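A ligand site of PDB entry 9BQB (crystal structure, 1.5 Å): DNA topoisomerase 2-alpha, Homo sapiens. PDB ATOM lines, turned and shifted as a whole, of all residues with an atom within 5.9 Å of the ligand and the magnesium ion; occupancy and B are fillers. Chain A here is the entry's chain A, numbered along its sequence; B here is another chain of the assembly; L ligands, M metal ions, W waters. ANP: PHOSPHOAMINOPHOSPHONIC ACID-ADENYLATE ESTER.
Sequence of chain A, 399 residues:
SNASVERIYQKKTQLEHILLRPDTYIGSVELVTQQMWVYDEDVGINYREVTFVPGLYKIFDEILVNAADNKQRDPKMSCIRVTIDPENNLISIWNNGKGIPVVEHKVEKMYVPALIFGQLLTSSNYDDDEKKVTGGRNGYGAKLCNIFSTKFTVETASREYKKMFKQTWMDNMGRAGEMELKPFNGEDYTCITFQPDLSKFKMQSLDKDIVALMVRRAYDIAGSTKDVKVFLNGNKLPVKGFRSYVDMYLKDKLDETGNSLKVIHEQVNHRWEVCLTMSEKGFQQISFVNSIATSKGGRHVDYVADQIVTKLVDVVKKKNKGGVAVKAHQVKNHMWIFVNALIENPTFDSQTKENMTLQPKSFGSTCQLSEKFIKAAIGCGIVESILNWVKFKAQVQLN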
ATOM      1  N   GLU A  62      -0.586   0.899 -12.128  1.00  0.00           N
ATOM      2  CA  GLU A  62      -1.581   0.716 -11.074  1.00  0.00           C
ATOM      3  C   GLU A  62      -1.263   1.598  -9.870  1.00  0.00           C
ATOM      4  O   GLU A  62      -2.173   2.202  -9.298  1.00  0.00           O
ATOM      5  CB  GLU A  62      -1.658  -0.755 -10.652  1.00  0.00           C
ATOM      6  CG  GLU A  62      -2.253  -1.729 -11.682  1.00  0.00           C
ATOM      7  CD  GLU A  62      -3.756  -1.570 -11.956  1.00  0.00           C
ATOM      8  OE1 GLU A  62      -4.294  -2.345 -12.781  1.00  0.00           O
ATOM      9  OE2 GLU A  62      -4.424  -0.678 -11.359  1.00  0.00           O
ATOM     10  N   ILE A  63       0.014   1.681  -9.481  1.00  0.00           N
ATOM     11  CA  ILE A  63       0.370   2.481  -8.305  1.00  0.00           C
ATOM     12  C   ILE A  63       0.299   3.972  -8.627  1.00  0.00           C
ATOM     13  O   ILE A  63      -0.088   4.784  -7.777  1.00  0.00           O
ATOM     14  CB  ILE A  63       1.772   2.075  -7.794  1.00  0.00           C
ATOM     15  CG1 ILE A  63       1.829   0.566  -7.496  1.00  0.00           C
ATOM     16  CG2 ILE A  63       2.178   2.898  -6.548  1.00  0.00           C
ATOM     17  CD1 ILE A  63       0.749   0.069  -6.531  1.00  0.00           C
ATOM     18  N   VAL A  65      -1.718   5.515 -10.852  1.00  0.00           N
ATOM     19  CA  VAL A  65      -3.121   5.925 -10.871  1.00  0.00           C
ATOM     20  C   VAL A  65      -3.696   5.963  -9.457  1.00  0.00           C
ATOM     21  O   VAL A  65      -4.507   6.835  -9.145  1.00  0.00           O
ATOM     22  CB  VAL A  65      -3.933   5.003 -11.797  1.00  0.00           C
ATOM     23  CG1 VAL A  65      -5.457   5.285 -11.714  1.00  0.00           C
ATOM     24  CG2 VAL A  65      -3.476   5.180 -13.240  1.00  0.00           C
ATOM     25  N   ASN A  66      -3.303   5.026  -8.594  1.00  0.00           N
ATOM     26  CA  ASN A  66      -3.757   5.077  -7.208  1.00  0.00           C
ATOM     27  C   ASN A  66      -3.376   6.399  -6.547  1.00  0.00           C
ATOM     28  O   ASN A  66      -4.128   6.931  -5.716  1.00  0.00           O
ATOM     29  CB  ASN A  66      -3.173   3.933  -6.378  1.00  0.00           C
ATOM     30  CG  ASN A  66      -3.911   2.620  -6.568  1.00  0.00           C
ATOM     31  OD1 ASN A  66      -5.019   2.573  -7.114  1.00  0.00           O
ATOM     32  ND2 ASN A  66      -3.327   1.540  -6.063  1.00  0.00           N
ATOM     33  N   ALA A  67      -2.195   6.926  -6.857  1.00  0.00           N
ATOM     34  CA  ALA A  67      -1.777   8.206  -6.295  1.00  0.00           C
ATOM     35  C   ALA A  67      -2.638   9.345  -6.832  1.00  0.00           C
ATOM     36  O   ALA A  67      -3.080  10.208  -6.068  1.00  0.00           O
ATOM     37  CB  ALA A  67      -0.303   8.453  -6.601  1.00  0.00           C
ATOM     38  N   ASP A  69      -5.641   9.064  -7.870  1.00  0.00           N
ATOM     39  CA  ASP A  69      -6.962   8.884  -7.262  1.00  0.00           C
ATOM     40  C   ASP A  69      -7.067   9.602  -5.920  1.00  0.00           C
ATOM     41  O   ASP A  69      -8.165  10.030  -5.530  1.00  0.00           O
ATOM     42  CB  ASP A  69      -7.252   7.392  -7.034  1.00  0.00           C
ATOM     43  CG  ASP A  69      -7.576   6.632  -8.309  1.00  0.00           C
ATOM     44  OD1 ASP A  69      -7.826   7.280  -9.343  1.00  0.00           O
ATOM     45  OD2 ASP A  69      -7.571   5.374  -8.275  1.00  0.00           O
ATOM     46  N   ASN A  70      -5.971   9.713  -5.187  1.00  0.00           N
ATOM     47  CA  ASN A  70      -6.089  10.342  -3.874  1.00  0.00           C
ATOM     48  C   ASN A  70      -6.420  11.826  -3.972  1.00  0.00           C
ATOM     49  O   ASN A  70      -6.872  12.419  -2.978  1.00  0.00           O
ATOM     50  CB  ASN A  70      -4.827  10.174  -3.046  1.00  0.00           C
ATOM     51  CG  ASN A  70      -5.106  10.268  -1.544  1.00  0.00           C
ATOM     52  OD1 ASN A  70      -5.977   9.548  -1.026  1.00  0.00           O
ATOM     53  ND2 ASN A  70      -4.404  11.152  -0.847  1.00  0.00           N
ATOM     54  N   ARG A  73     -10.061  11.910  -3.622  1.00  0.00           N
ATOM     55  CA  ARG A  73     -10.413  11.639  -2.235  1.00  0.00           C
ATOM     56  C   ARG A  73     -10.133  12.848  -1.343  1.00  0.00           C
ATOM     57  O   ARG A  73     -10.949  13.182  -0.462  1.00  0.00           O
ATOM     58  CB  ARG A  73      -9.633  10.424  -1.746  1.00  0.00           C
ATOM     59  CG  ARG A  73      -9.733  10.161  -0.258  1.00  0.00           C
ATOM     60  CD  ARG A  73      -9.193   8.780   0.078  1.00  0.00           C
ATOM     61  NE  ARG A  73      -9.143   8.512   1.511  1.00  0.00           N
ATOM     62  CZ  ARG A  73      -8.029   8.593   2.253  1.00  0.00           C
ATOM     63  NH1 ARG A  73      -6.877   8.937   1.693  1.00  0.00           N
ATOM     64  NH2 ARG A  73      -8.090   8.314   3.540  1.00  0.00           N
ATOM     65  N   ASN A  95       2.764  10.329  -2.501  1.00  0.00           N
ATOM     66  CA  ASN A  95       1.779  11.382  -2.668  1.00  0.00           C
ATOM     67  C   ASN A  95       1.447  11.966  -1.294  1.00  0.00           C
ATOM     68  O   ASN A  95       1.628  11.313  -0.276  1.00  0.00           O
ATOM     69  CB  ASN A  95       0.489  10.879  -3.333  1.00  0.00           C
ATOM     70  CG  ASN A  95      -0.269   9.921  -2.462  1.00  0.00           C
ATOM     71  OD1 ASN A  95      -0.107   8.703  -2.550  1.00  0.00           O
ATOM     72  ND2 ASN A  95      -1.107  10.450  -1.580  1.00  0.00           N
ATOM     73  N   LYS A  98      -4.498  13.149   2.319  1.00  0.00           N
ATOM     74  CA  LYS A  98      -4.891  12.230   3.389  1.00  0.00           C
ATOM     75  C   LYS A  98      -4.280  10.837   3.243  1.00  0.00           C
ATOM     76  O   LYS A  98      -4.368  10.214   2.185  1.00  0.00           O
ATOM     77  CB  LYS A  98      -6.416  12.131   3.396  1.00  0.00           C
ATOM     78  CG  LYS A  98      -7.042  11.509   4.612  1.00  0.00           C
ATOM     79  CD  LYS A  98      -8.510  11.938   4.720  1.00  0.00           C
ATOM     80  CE  LYS A  98      -9.220  11.220   5.853  1.00  0.00           C
ATOM     81  NZ  LYS A  98      -8.432  11.265   7.116  1.00  0.00           N
ATOM     82  N   GLY A  99      -3.676  10.356   4.336  1.00  0.00           N
ATOM     83  CA  GLY A  99      -3.179   8.999   4.375  1.00  0.00           C
ATOM     84  C   GLY A  99      -4.284   8.000   4.596  1.00  0.00           C
ATOM     85  O   GLY A  99      -5.451   8.331   4.788  1.00  0.00           O
ATOM     86  N   ILE A 100      -3.916   6.726   4.540  1.00  0.00           N
ATOM     87  CA  ILE A 100      -4.886   5.653   4.768  1.00  0.00           C
ATOM     88  C   ILE A 100      -5.081   5.526   6.267  1.00  0.00           C
ATOM     89  O   ILE A 100      -4.087   5.633   7.012  1.00  0.00           O
ATOM     90  CB  ILE A 100      -4.403   4.342   4.143  1.00  0.00           C
ATOM     91  CG1 ILE A 100      -4.280   4.530   2.641  1.00  0.00           C
ATOM     92  CG2 ILE A 100      -5.341   3.210   4.460  1.00  0.00           C
ATOM     93  CD1 ILE A 100      -3.298   3.606   2.029  1.00  0.00           C
ATOM     94  N   ILE A 116      -5.846  -3.678   2.520  1.00  0.00           N
ATOM     95  CA  ILE A 116      -6.110  -3.251   1.148  1.00  0.00           C
ATOM     96  C   ILE A 116      -4.882  -3.302   0.251  1.00  0.00           C
ATOM     97  O   ILE A 116      -5.025  -3.104  -0.970  1.00  0.00           O
ATOM     98  CB  ILE A 116      -6.744  -1.844   1.157  1.00  0.00           C
ATOM     99  CG1 ILE A 116      -5.768  -0.767   1.632  1.00  0.00           C
ATOM    100  CG2 ILE A 116      -7.985  -1.837   2.061  1.00  0.00           C
ATOM    101  CD1 ILE A 116      -6.386   0.647   1.742  1.00  0.00           C
ATOM    102  N   PHE A 117      -3.693  -3.593   0.785  1.00  0.00           N
ATOM    103  CA  PHE A 117      -2.531  -3.848  -0.053  1.00  0.00           C
ATOM    104  C   PHE A 117      -2.098  -5.324  -0.059  1.00  0.00           C
ATOM    105  O   PHE A 117      -1.297  -5.707  -0.924  1.00  0.00           O
ATOM    106  CB  PHE A 117      -1.342  -2.980   0.380  1.00  0.00           C
ATOM    107  CG  PHE A 117      -1.472  -1.536  -0.016  1.00  0.00           C
ATOM    108  CD1 PHE A 117      -1.071  -1.119  -1.276  1.00  0.00           C
ATOM    109  CD2 PHE A 117      -2.021  -0.598   0.851  1.00  0.00           C
ATOM    110  CE1 PHE A 117      -1.200   0.197  -1.674  1.00  0.00           C
ATOM    111  CE2 PHE A 117      -2.155   0.742   0.454  1.00  0.00           C
ATOM    112  CZ  PHE A 117      -1.749   1.134  -0.807  1.00  0.00           C
ATOM    113  N   THR A 122     -10.096  -6.041  -2.391  1.00  0.00           N
ATOM    114  CA  THR A 122     -10.273  -5.059  -1.321  1.00  0.00           C
ATOM    115  C   THR A 122     -10.244  -3.658  -1.920  1.00  0.00           C
ATOM    116  O   THR A 122      -9.323  -3.334  -2.688  1.00  0.00           O
ATOM    117  CB  THR A 122      -9.202  -5.210  -0.229  1.00  0.00           C
ATOM    118  OG1 THR A 122      -7.894  -5.196  -0.817  1.00  0.00           O
ATOM    119  CG2 THR A 122      -9.392  -6.523   0.564  1.00  0.00           C
ATOM    120  N   SER A 123     -11.211  -2.832  -1.548  1.00  0.00           N
ATOM    121  CA  SER A 123     -11.360  -1.553  -2.251  1.00  0.00           C
ATOM    122  C   SER A 123     -12.278  -0.627  -1.474  1.00  0.00           C
ATOM    123  O   SER A 123     -13.157  -1.062  -0.726  1.00  0.00           O
ATOM    124  CB  SER A 123     -11.938  -1.758  -3.658  1.00  0.00           C
ATOM    125  OG  SER A 123     -12.026  -0.541  -4.384  1.00  0.00           O
ATOM    126  N   SER A 124     -12.093   0.678  -1.712  1.00  0.00           N
ATOM    127  CA  SER A 124     -13.058   1.698  -1.311  1.00  0.00           C
ATOM    128  C   SER A 124     -14.029   2.074  -2.430  1.00  0.00           C
ATOM    129  O   SER A 124     -14.879   2.963  -2.232  1.00  0.00           O
ATOM    130  CB  SER A 124     -12.322   2.957  -0.827  1.00  0.00           C
ATOM    131  OG  SER A 124     -11.482   3.532  -1.817  1.00  0.00           O
ATOM    132  N   ASN A 125     -13.971   1.375  -3.562  1.00  0.00           N
ATOM    133  CA  ASN A 125     -14.736   1.707  -4.759  1.00  0.00           C
ATOM    134  C   ASN A 125     -15.827   0.700  -5.065  1.00  0.00           C
ATOM    135  O   ASN A 125     -16.301   0.646  -6.215  1.00  0.00           O
ATOM    136  CB  ASN A 125     -13.774   1.844  -5.927  1.00  0.00           C
ATOM    137  CG  ASN A 125     -12.915   3.055  -5.808  1.00  0.00           C
ATOM    138  OD1 ASN A 125     -13.437   4.175  -5.788  1.00  0.00           O
ATOM    139  ND2 ASN A 125     -11.601   2.867  -5.645  1.00  0.00           N
ATOM    140  N   GLY A 135     -10.066   6.433 -10.740  1.00  0.00           N
ATOM    141  CA  GLY A 135      -9.777   5.346 -11.661  1.00  0.00           C
ATOM    142  C   GLY A 135      -9.961   3.968 -11.067  1.00  0.00           C
ATOM    143  O   GLY A 135     -10.187   3.000 -11.800  1.00  0.00           O
ATOM    144  N   GLY A 136      -9.880   3.857  -9.738  1.00  0.00           N
ATOM    145  CA  GLY A 136     -10.040   2.569  -9.089  1.00  0.00           C
ATOM    146  C   GLY A 136     -11.466   2.050  -9.137  1.00  0.00           C
ATOM    147  O   GLY A 136     -12.427   2.782  -8.887  1.00  0.00           O
ATOM    148  N   ARG A 137     -11.587   0.762  -9.472  1.00  0.00           N
ATOM    149  CA  ARG A 137     -12.899   0.136  -9.593  1.00  0.00           C
ATOM    150  C   ARG A 137     -12.959  -1.261  -8.974  1.00  0.00           C
ATOM    151  O   ARG A 137     -13.968  -1.599  -8.361  1.00  0.00           O
ATOM    152  CB  ARG A 137     -13.288   0.047 -11.084  1.00  0.00           C
ATOM    153  CG  ARG A 137     -13.363   1.404 -11.799  1.00  0.00           C
ATOM    154  CD  ARG A 137     -14.532   2.305 -11.307  1.00  0.00           C
ATOM    155  NE  ARG A 137     -15.810   1.633 -11.564  1.00  0.00           N
ATOM    156  CZ  ARG A 137     -16.795   1.450 -10.683  1.00  0.00           C
ATOM    157  NH1 ARG A 137     -16.723   1.937  -9.459  1.00  0.00           N
ATOM    158  NH2 ARG A 137     -17.871   0.773 -11.055  1.00  0.00           N
ATOM    159  N   ASN A 138     -11.907  -2.075  -9.114  1.00  0.00           N
ATOM    160  CA  ASN A 138     -12.056  -3.512  -8.931  1.00  0.00           C
ATOM    161  C   ASN A 138     -11.421  -4.110  -7.677  1.00  0.00           C
ATOM    162  O   ASN A 138     -11.746  -5.255  -7.340  1.00  0.00           O
ATOM    163  CB  ASN A 138     -11.470  -4.257 -10.137  1.00  0.00           C
ATOM    164  CG  ASN A 138     -12.070  -3.795 -11.438  1.00  0.00           C
ATOM    165  OD1 ASN A 138     -13.306  -3.694 -11.553  1.00  0.00           O
ATOM    166  ND2 ASN A 138     -11.223  -3.470 -12.406  1.00  0.00           N
ATOM    167  N   GLY A 139     -10.533  -3.388  -6.989  1.00  0.00           N
ATOM    168  CA  GLY A 139      -9.882  -3.905  -5.791  1.00  0.00           C
ATOM    169  C   GLY A 139      -8.722  -4.847  -6.040  1.00  0.00           C
ATOM    170  O   GLY A 139      -8.425  -5.667  -5.164  1.00  0.00           O
ATOM    171  N   TYR A 140      -8.067  -4.756  -7.201  1.00  0.00           N
ATOM    172  CA  TYR A 140      -6.956  -5.606  -7.594  1.00  0.00           C
ATOM    173  C   TYR A 140      -5.616  -4.881  -7.702  1.00  0.00           C
ATOM    174  O   TYR A 140      -4.594  -5.440  -7.318  1.00  0.00           O
ATOM    175  CB  TYR A 140      -7.245  -6.221  -8.967  1.00  0.00           C
ATOM    176  CG  TYR A 140      -7.852  -7.594  -9.001  1.00  0.00           C
ATOM    177  CD1 TYR A 140      -7.192  -8.681  -8.474  1.00  0.00           C
ATOM    178  CD2 TYR A 140      -9.092  -7.818  -9.615  1.00  0.00           C
ATOM    179  CE1 TYR A 140      -7.734  -9.936  -8.533  1.00  0.00           C
ATOM    180  CE2 TYR A 140      -9.633  -9.085  -9.682  1.00  0.00           C
ATOM    181  CZ  TYR A 140      -8.945 -10.138  -9.130  1.00  0.00           C
ATOM    182  OH  TYR A 140      -9.455 -11.413  -9.171  1.00  0.00           O
ATOM    183  N   GLY A 141      -5.615  -3.651  -8.229  1.00  0.00           N
ATOM    184  CA  GLY A 141      -4.408  -3.075  -8.797  1.00  0.00           C
ATOM    185  C   GLY A 141      -3.171  -3.129  -7.910  1.00  0.00           C
ATOM    186  O   GLY A 141      -2.082  -3.515  -8.359  1.00  0.00           O
ATOM    187  N   ALA A 142      -3.314  -2.678  -6.656  1.00  0.00           N
ATOM    188  CA  ALA A 142      -2.158  -2.611  -5.762  1.00  0.00           C
ATOM    189  C   ALA A 142      -1.665  -4.003  -5.406  1.00  0.00           C
ATOM    190  O   ALA A 142      -0.450  -4.242  -5.292  1.00  0.00           O
ATOM    191  CB  ALA A 142      -2.525  -1.829  -4.504  1.00  0.00           C
ATOM    192  N   LYS A 143      -2.588  -4.944  -5.210  1.00  0.00           N
ATOM    193  CA  LYS A 143      -2.194  -6.322  -4.958  1.00  0.00           C
ATOM    194  C   LYS A 143      -1.515  -6.944  -6.169  1.00  0.00           C
ATOM    195  O   LYS A 143      -0.628  -7.783  -6.016  1.00  0.00           O
ATOM    196  CB  LYS A 143      -3.401  -7.170  -4.556  1.00  0.00           C
ATOM    197  CG  LYS A 143      -3.823  -7.033  -3.080  1.00  0.00           C
ATOM    198  CD  LYS A 143      -4.469  -5.684  -2.756  1.00  0.00           C
ATOM    199  CE  LYS A 143      -5.817  -5.476  -3.450  1.00  0.00           C
ATOM    200  NZ  LYS A 143      -6.490  -4.184  -3.082  1.00  0.00           N
ATOM    201  N   THR A 190       1.444   9.025   1.621  1.00  0.00           N
ATOM    202  CA  THR A 190       1.566   7.591   1.345  1.00  0.00           C
ATOM    203  C   THR A 190       2.726   7.412   0.374  1.00  0.00           C
ATOM    204  O   THR A 190       2.885   8.184  -0.568  1.00  0.00           O
ATOM    205  CB  THR A 190       0.265   7.020   0.755  1.00  0.00           C
ATOM    206  OG1 THR A 190      -0.778   7.105   1.742  1.00  0.00           O
ATOM    207  CG2 THR A 190       0.442   5.546   0.304  1.00  0.00           C
ATOM    208  N   ILE A 192       4.634   4.169  -1.745  1.00  0.00           N
ATOM    209  CA  ILE A 192       4.693   2.770  -2.165  1.00  0.00           C
ATOM    210  C   ILE A 192       6.040   2.542  -2.859  1.00  0.00           C
ATOM    211  O   ILE A 192       6.338   3.185  -3.870  1.00  0.00           O
ATOM    212  CB  ILE A 192       3.511   2.417  -3.097  1.00  0.00           C
ATOM    213  CG1 ILE A 192       2.171   2.858  -2.491  1.00  0.00           C
ATOM    214  CG2 ILE A 192       3.564   0.927  -3.488  1.00  0.00           C
ATOM    215  CD1 ILE A 192       1.842   2.231  -1.139  1.00  0.00           C
ATOM    216  N   GLN A 351      -9.152  -5.609 -16.502  1.00  0.00           N
ATOM    217  CA  GLN A 351      -8.451  -4.929 -15.420  1.00  0.00           C
ATOM    218  C   GLN A 351      -7.468  -3.883 -15.929  1.00  0.00           C
ATOM    219  O   GLN A 351      -7.176  -2.919 -15.208  1.00  0.00           O
ATOM    220  CB  GLN A 351      -7.716  -5.953 -14.551  1.00  0.00           C
ATOM    221  CG  GLN A 351      -6.834  -5.362 -13.449  1.00  0.00           C
ATOM    222  CD  GLN A 351      -7.616  -4.601 -12.377  1.00  0.00           C
ATOM    223  OE1 GLN A 351      -8.759  -4.923 -12.083  1.00  0.00           O
ATOM    224  NE2 GLN A 351      -6.984  -3.584 -11.793  1.00  0.00           N
ATOM    225  N   LYS A 353      -7.856  -1.725 -18.256  1.00  0.00           N
ATOM    226  CA  LYS A 353      -8.619  -0.489 -18.439  1.00  0.00           C
ATOM    227  C   LYS A 353      -8.145   0.319 -19.661  1.00  0.00           C
ATOM    228  O   LYS A 353      -8.061   1.555 -19.632  1.00  0.00           O
ATOM    229  CB  LYS A 353      -8.584   0.380 -17.170  1.00  0.00           C
ATOM    230  CG  LYS A 353      -9.142  -0.316 -15.925  1.00  0.00           C
ATOM    231  CD  LYS A 353      -8.923   0.545 -14.694  1.00  0.00           C
ATOM    232  CE  LYS A 353      -9.026  -0.188 -13.392  1.00  0.00           C
ATOM    233  NZ  LYS A 353      -8.637   0.694 -12.233  1.00  0.00           N
ATOM    234  N   TYR B   9     -13.980   0.602   3.426  1.00  0.00           N
ATOM    235  CA  TYR B   9     -13.045  -0.386   2.897  1.00  0.00           C
ATOM    236  C   TYR B   9     -13.637  -1.772   3.057  1.00  0.00           C
ATOM    237  O   TYR B   9     -13.853  -2.234   4.187  1.00  0.00           O
ATOM    238  CB  TYR B   9     -11.703  -0.287   3.612  1.00  0.00           C
ATOM    239  CG  TYR B   9     -11.028   1.052   3.489  1.00  0.00           C
ATOM    240  CD1 TYR B   9     -10.293   1.387   2.353  1.00  0.00           C
ATOM    241  CD2 TYR B   9     -11.116   1.995   4.508  1.00  0.00           C
ATOM    242  CE1 TYR B   9      -9.660   2.609   2.237  1.00  0.00           C
ATOM    243  CE2 TYR B   9     -10.498   3.226   4.405  1.00  0.00           C
ATOM    244  CZ  TYR B   9      -9.760   3.520   3.271  1.00  0.00           C
ATOM    245  OH  TYR B   9      -9.144   4.734   3.170  1.00  0.00           O
HETATM  246  PG  ANP L   1      -8.423  -1.124  -9.141  1.00  0.00           P
HETATM  247  O1G ANP L   1      -7.120  -0.389  -9.181  1.00  0.00           O
HETATM  248  O2G ANP L   1      -9.374  -0.799 -10.344  1.00  0.00           O
HETATM  249  O3G ANP L   1      -8.208  -2.681  -9.037  1.00  0.00           O
HETATM  250  PB  ANP L   1      -8.678   0.095  -6.459  1.00  0.00           P
HETATM  251  O1B ANP L   1      -7.798   1.242  -6.814  1.00  0.00           O
HETATM  252  O2B ANP L   1      -9.906   0.445  -5.544  1.00  0.00           O
HETATM  253  N3B ANP L   1      -9.343  -0.655  -7.807  1.00  0.00           N
HETATM  254  PA  ANP L   1      -6.275  -1.018  -5.419  1.00  0.00           P
HETATM  255  O1A ANP L   1      -5.493  -0.343  -6.481  1.00  0.00           O
HETATM  256  O2A ANP L   1      -5.865  -2.465  -5.133  1.00  0.00           O
HETATM  257  O3A ANP L   1      -7.838  -1.014  -5.746  1.00  0.00           O
HETATM  258  O5' ANP L   1      -6.188  -0.132  -4.095  1.00  0.00           O
HETATM  259  C5' ANP L   1      -6.857  -0.606  -2.921  1.00  0.00           C
HETATM  260  C4' ANP L   1      -7.368   0.549  -2.109  1.00  0.00           C
HETATM  261  O4' ANP L   1      -6.256   1.183  -1.450  1.00  0.00           O
HETATM  262  C3' ANP L   1      -8.032   1.647  -2.911  1.00  0.00           C
HETATM  263  O3' ANP L   1      -9.423   1.370  -3.083  1.00  0.00           O
HETATM  264  C2' ANP L   1      -7.802   2.889  -2.045  1.00  0.00           C
HETATM  265  O2' ANP L   1      -8.815   3.012  -1.042  1.00  0.00           O
HETATM  266  C1' ANP L   1      -6.482   2.575  -1.335  1.00  0.00           C
HETATM  267  N9  ANP L   1      -5.298   3.269  -1.853  1.00  0.00           N
HETATM  268  C8  ANP L   1      -4.384   2.810  -2.762  1.00  0.00           C
HETATM  269  N7  ANP L   1      -3.402   3.640  -3.009  1.00  0.00           N
HETATM  270  C5  ANP L   1      -3.686   4.724  -2.182  1.00  0.00           C
HETATM  271  C6  ANP L   1      -3.019   5.943  -1.967  1.00  0.00           C
HETATM  272  N6  ANP L   1      -1.899   6.296  -2.597  1.00  0.00           N
HETATM  273  N1  ANP L   1      -3.565   6.800  -1.075  1.00  0.00           N
HETATM  274  C2  ANP L   1      -4.692   6.442  -0.449  1.00  0.00           C
HETATM  275  N3  ANP L   1      -5.404   5.331  -0.565  1.00  0.00           N
HETATM  276  C4  ANP L   1      -4.847   4.500  -1.463  1.00  0.00           C
HETATM  277 MG    MG M   1      -6.112   1.023  -7.996  1.00  0.00          MG
HETATM  278  O   HOH W   1      -0.097   5.023  -4.821  1.00  0.00           O
HETATM  279  O   HOH W   2      -7.291   7.402  -2.651  1.00  0.00           O
HETATM  280  O   HOH W   3      -6.718   2.553  -9.370  1.00  0.00           O
HETATM  281  O   HOH W   4      -7.924   5.405   0.827  1.00  0.00           O
HETATM  282  O   HOH W   5      -2.507   8.822   0.594  1.00  0.00           O
HETATM  283  O   HOH W   6      -7.604   4.023  -5.958  1.00  0.00           O
HETATM  284  O   HOH W   7      -1.074   2.437  -4.297  1.00  0.00           O
HETATM  285  O   HOH W   8      -6.014   5.495  -4.252  1.00  0.00           O
HETATM  286  O   HOH W   9     -10.362   5.718  -0.580  1.00  0.00           O
HETATM  287  O   HOH W  10      -4.407   0.604  -9.101  1.00  0.00           O
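The side-chain hydroxyl (OG) of Ser 123 sits at hydrogen-bond distance from an oxygen (O2B) of the ligand.
The side-chain amide oxygen (OD1) of Asn 95 lies within hydrogen-bond range of a nitrogen (N6) of the ligand, 3.0 Å away.
O3G of the ligand is in hydrogen-bond range of N of Tyr 140 (2.8 Å).
The backbone NH (N) of Gly 139 lies within hydrogen-bond range of an oxygen (O3G) of the ligand, at 3.2 Å.
N of Gly 141 is in hydrogen-bond range of O3G of the ligand, 2.9 Å away.
An oxygen (O2G) of the ligand lies within hydrogen-bond range of the backbone NH of Arg 137, at 2.8 Å.
An oxygen (O3') of the ligand is in hydrogen-bond range of the backbone NH of Ser 124, at 3.1 Å.
The backbone NH (N) of Asn 138 lies within hydrogen-bond range of an oxygen (O2G) of the ligand (3.1 Å).
NZ of Lys 143 is in salt-bridge range of O2A of the ligand (2.7 Å).
The side-chain hydroxyl of Ser 124 lies within hydrogen-bond range of an oxygen (O2') of the ligand, at 2.8 Å.
The side-chain amide nitrogen of Gln 351 lies within hydrogen-bond range of an oxygen (O3G) of the ligand (3.1 Å).
An oxygen (O2A) of the ligand sits at hydrogen-bond distance from the backbone NH of Ala 142.
An oxygen (O2G) of the ligand lies within salt-bridge range of the side-chain amino group of Lys 353, 2.5 Å away.
The side-chain amide nitrogen (ND2) of Asn 125 is in hydrogen-bond range of an oxygen (O2B) of the ligand (3.0 Å).
The side-chain amino group of Lys 143 lies within hydrogen-bond range of the side-chain hydroxyl of Thr 122 (2.9 Å).
O of Gly 135 sits at hydrogen-bond distance from NZ of Lys 353 (2.8 Å).
The side-chain amide oxygen (OD1) of Asn 70 lies within hydrogen-bond range of the guanidinium group (NH1) of Arg 73, 2.9 Å away.
O of Gly 139 lies within hydrogen-bond range of N of Thr 122, at 3.3 Å.
NZ of Lys 143 sits at hydrogen-bond distance from O of Ile 116 (2.8 Å).
ND2 of Asn 66 sits close to O of Glu 62 (3.5 Å).
The side-chain amide nitrogen (ND2) of Asn 95 sits close to the side-chain amide nitrogen (ND2) of Asn 70.
NH2 of Arg 73 is in hydrogen-bond range of O of Gly 99 (2.9 Å).
The side-chain carboxylate (OE2) of Glu 62 lies close to an oxygen (O1G) of the ligand (3.5 Å).
Asn 70 touches the ligand (OD1 to C2, 3.4 Å).
Arg 73 touches the ligand (NH1 to C2, 3.9 Å).
Ile 100 touches the ligand (CG1 to N3, 3.5 Å).
CD1 of Ile 116 touches O4' of the ligand, 3.2 Å away.
CZ of Phe 117 touches C8 of the ligand, at 3.7 Å.
Thr 122 touches the ligand.
CA of Gly 136 touches O1B of the ligand, 3.5 Å away.
CG2 of Thr 190 touches N6 of the ligand (3.8 Å).
CE1 of Tyr 9 of chain B touches O2' of the ligand, at 3.4 Å.
Within 4 Å of the ligand: Glu 62, Asn 66, Asn 70, Arg 73, Asn 95, Ile 100, Ile 116, Phe 117, Thr 122, Ser 123, Ser 124, Asn 125, Gly 136, Arg 137, Asn 138, Gly 139, Tyr 140, Gly 141, Ala 142, Lys 143, Thr 190, Gln 351, Lys 353 and Tyr 9 of chain B.
One residue has an atom within 4 Å of the magnesium ion: Asn 66.
The magnesium ion is bound by an oxygen (O1B) of the ligand, water W10, the side-chain amide oxygen of Asn 66, an oxygen (O1G) of the ligand, an oxygen (O1A) of the ligand and water W3.
The magnesium ion has six donor atoms within binding distance.
Water W10 bridges OE2 of Glu 62 and ND2 of Asn 66.
Water W3 lies within hydrogen-bond range of the side-chain carboxylate (OD2) of Asp 69 and the backbone NH (N) of Gly 136.
Water W4 lies within hydrogen-bond range of OH of Tyr 9 of chain B (2.7 Å), N3 of the ligand (2.9 Å) and NE of Arg 73 (3.4 Å).
Water W1 lies within hydrogen-bond range of the backbone carbonyl oxygen (O) of Ile 63, a nitrogen (N6) of the ligand and the backbone NH (N) of Ala 67.
Water W8 bridges O of Asn 66 (2.8 Å) and N7 of the ligand (3.4 Å).
Water W2 lies within hydrogen-bond range of OD1 of Asn 70 (3.0 Å) and N3 of the ligand (3.5 Å).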
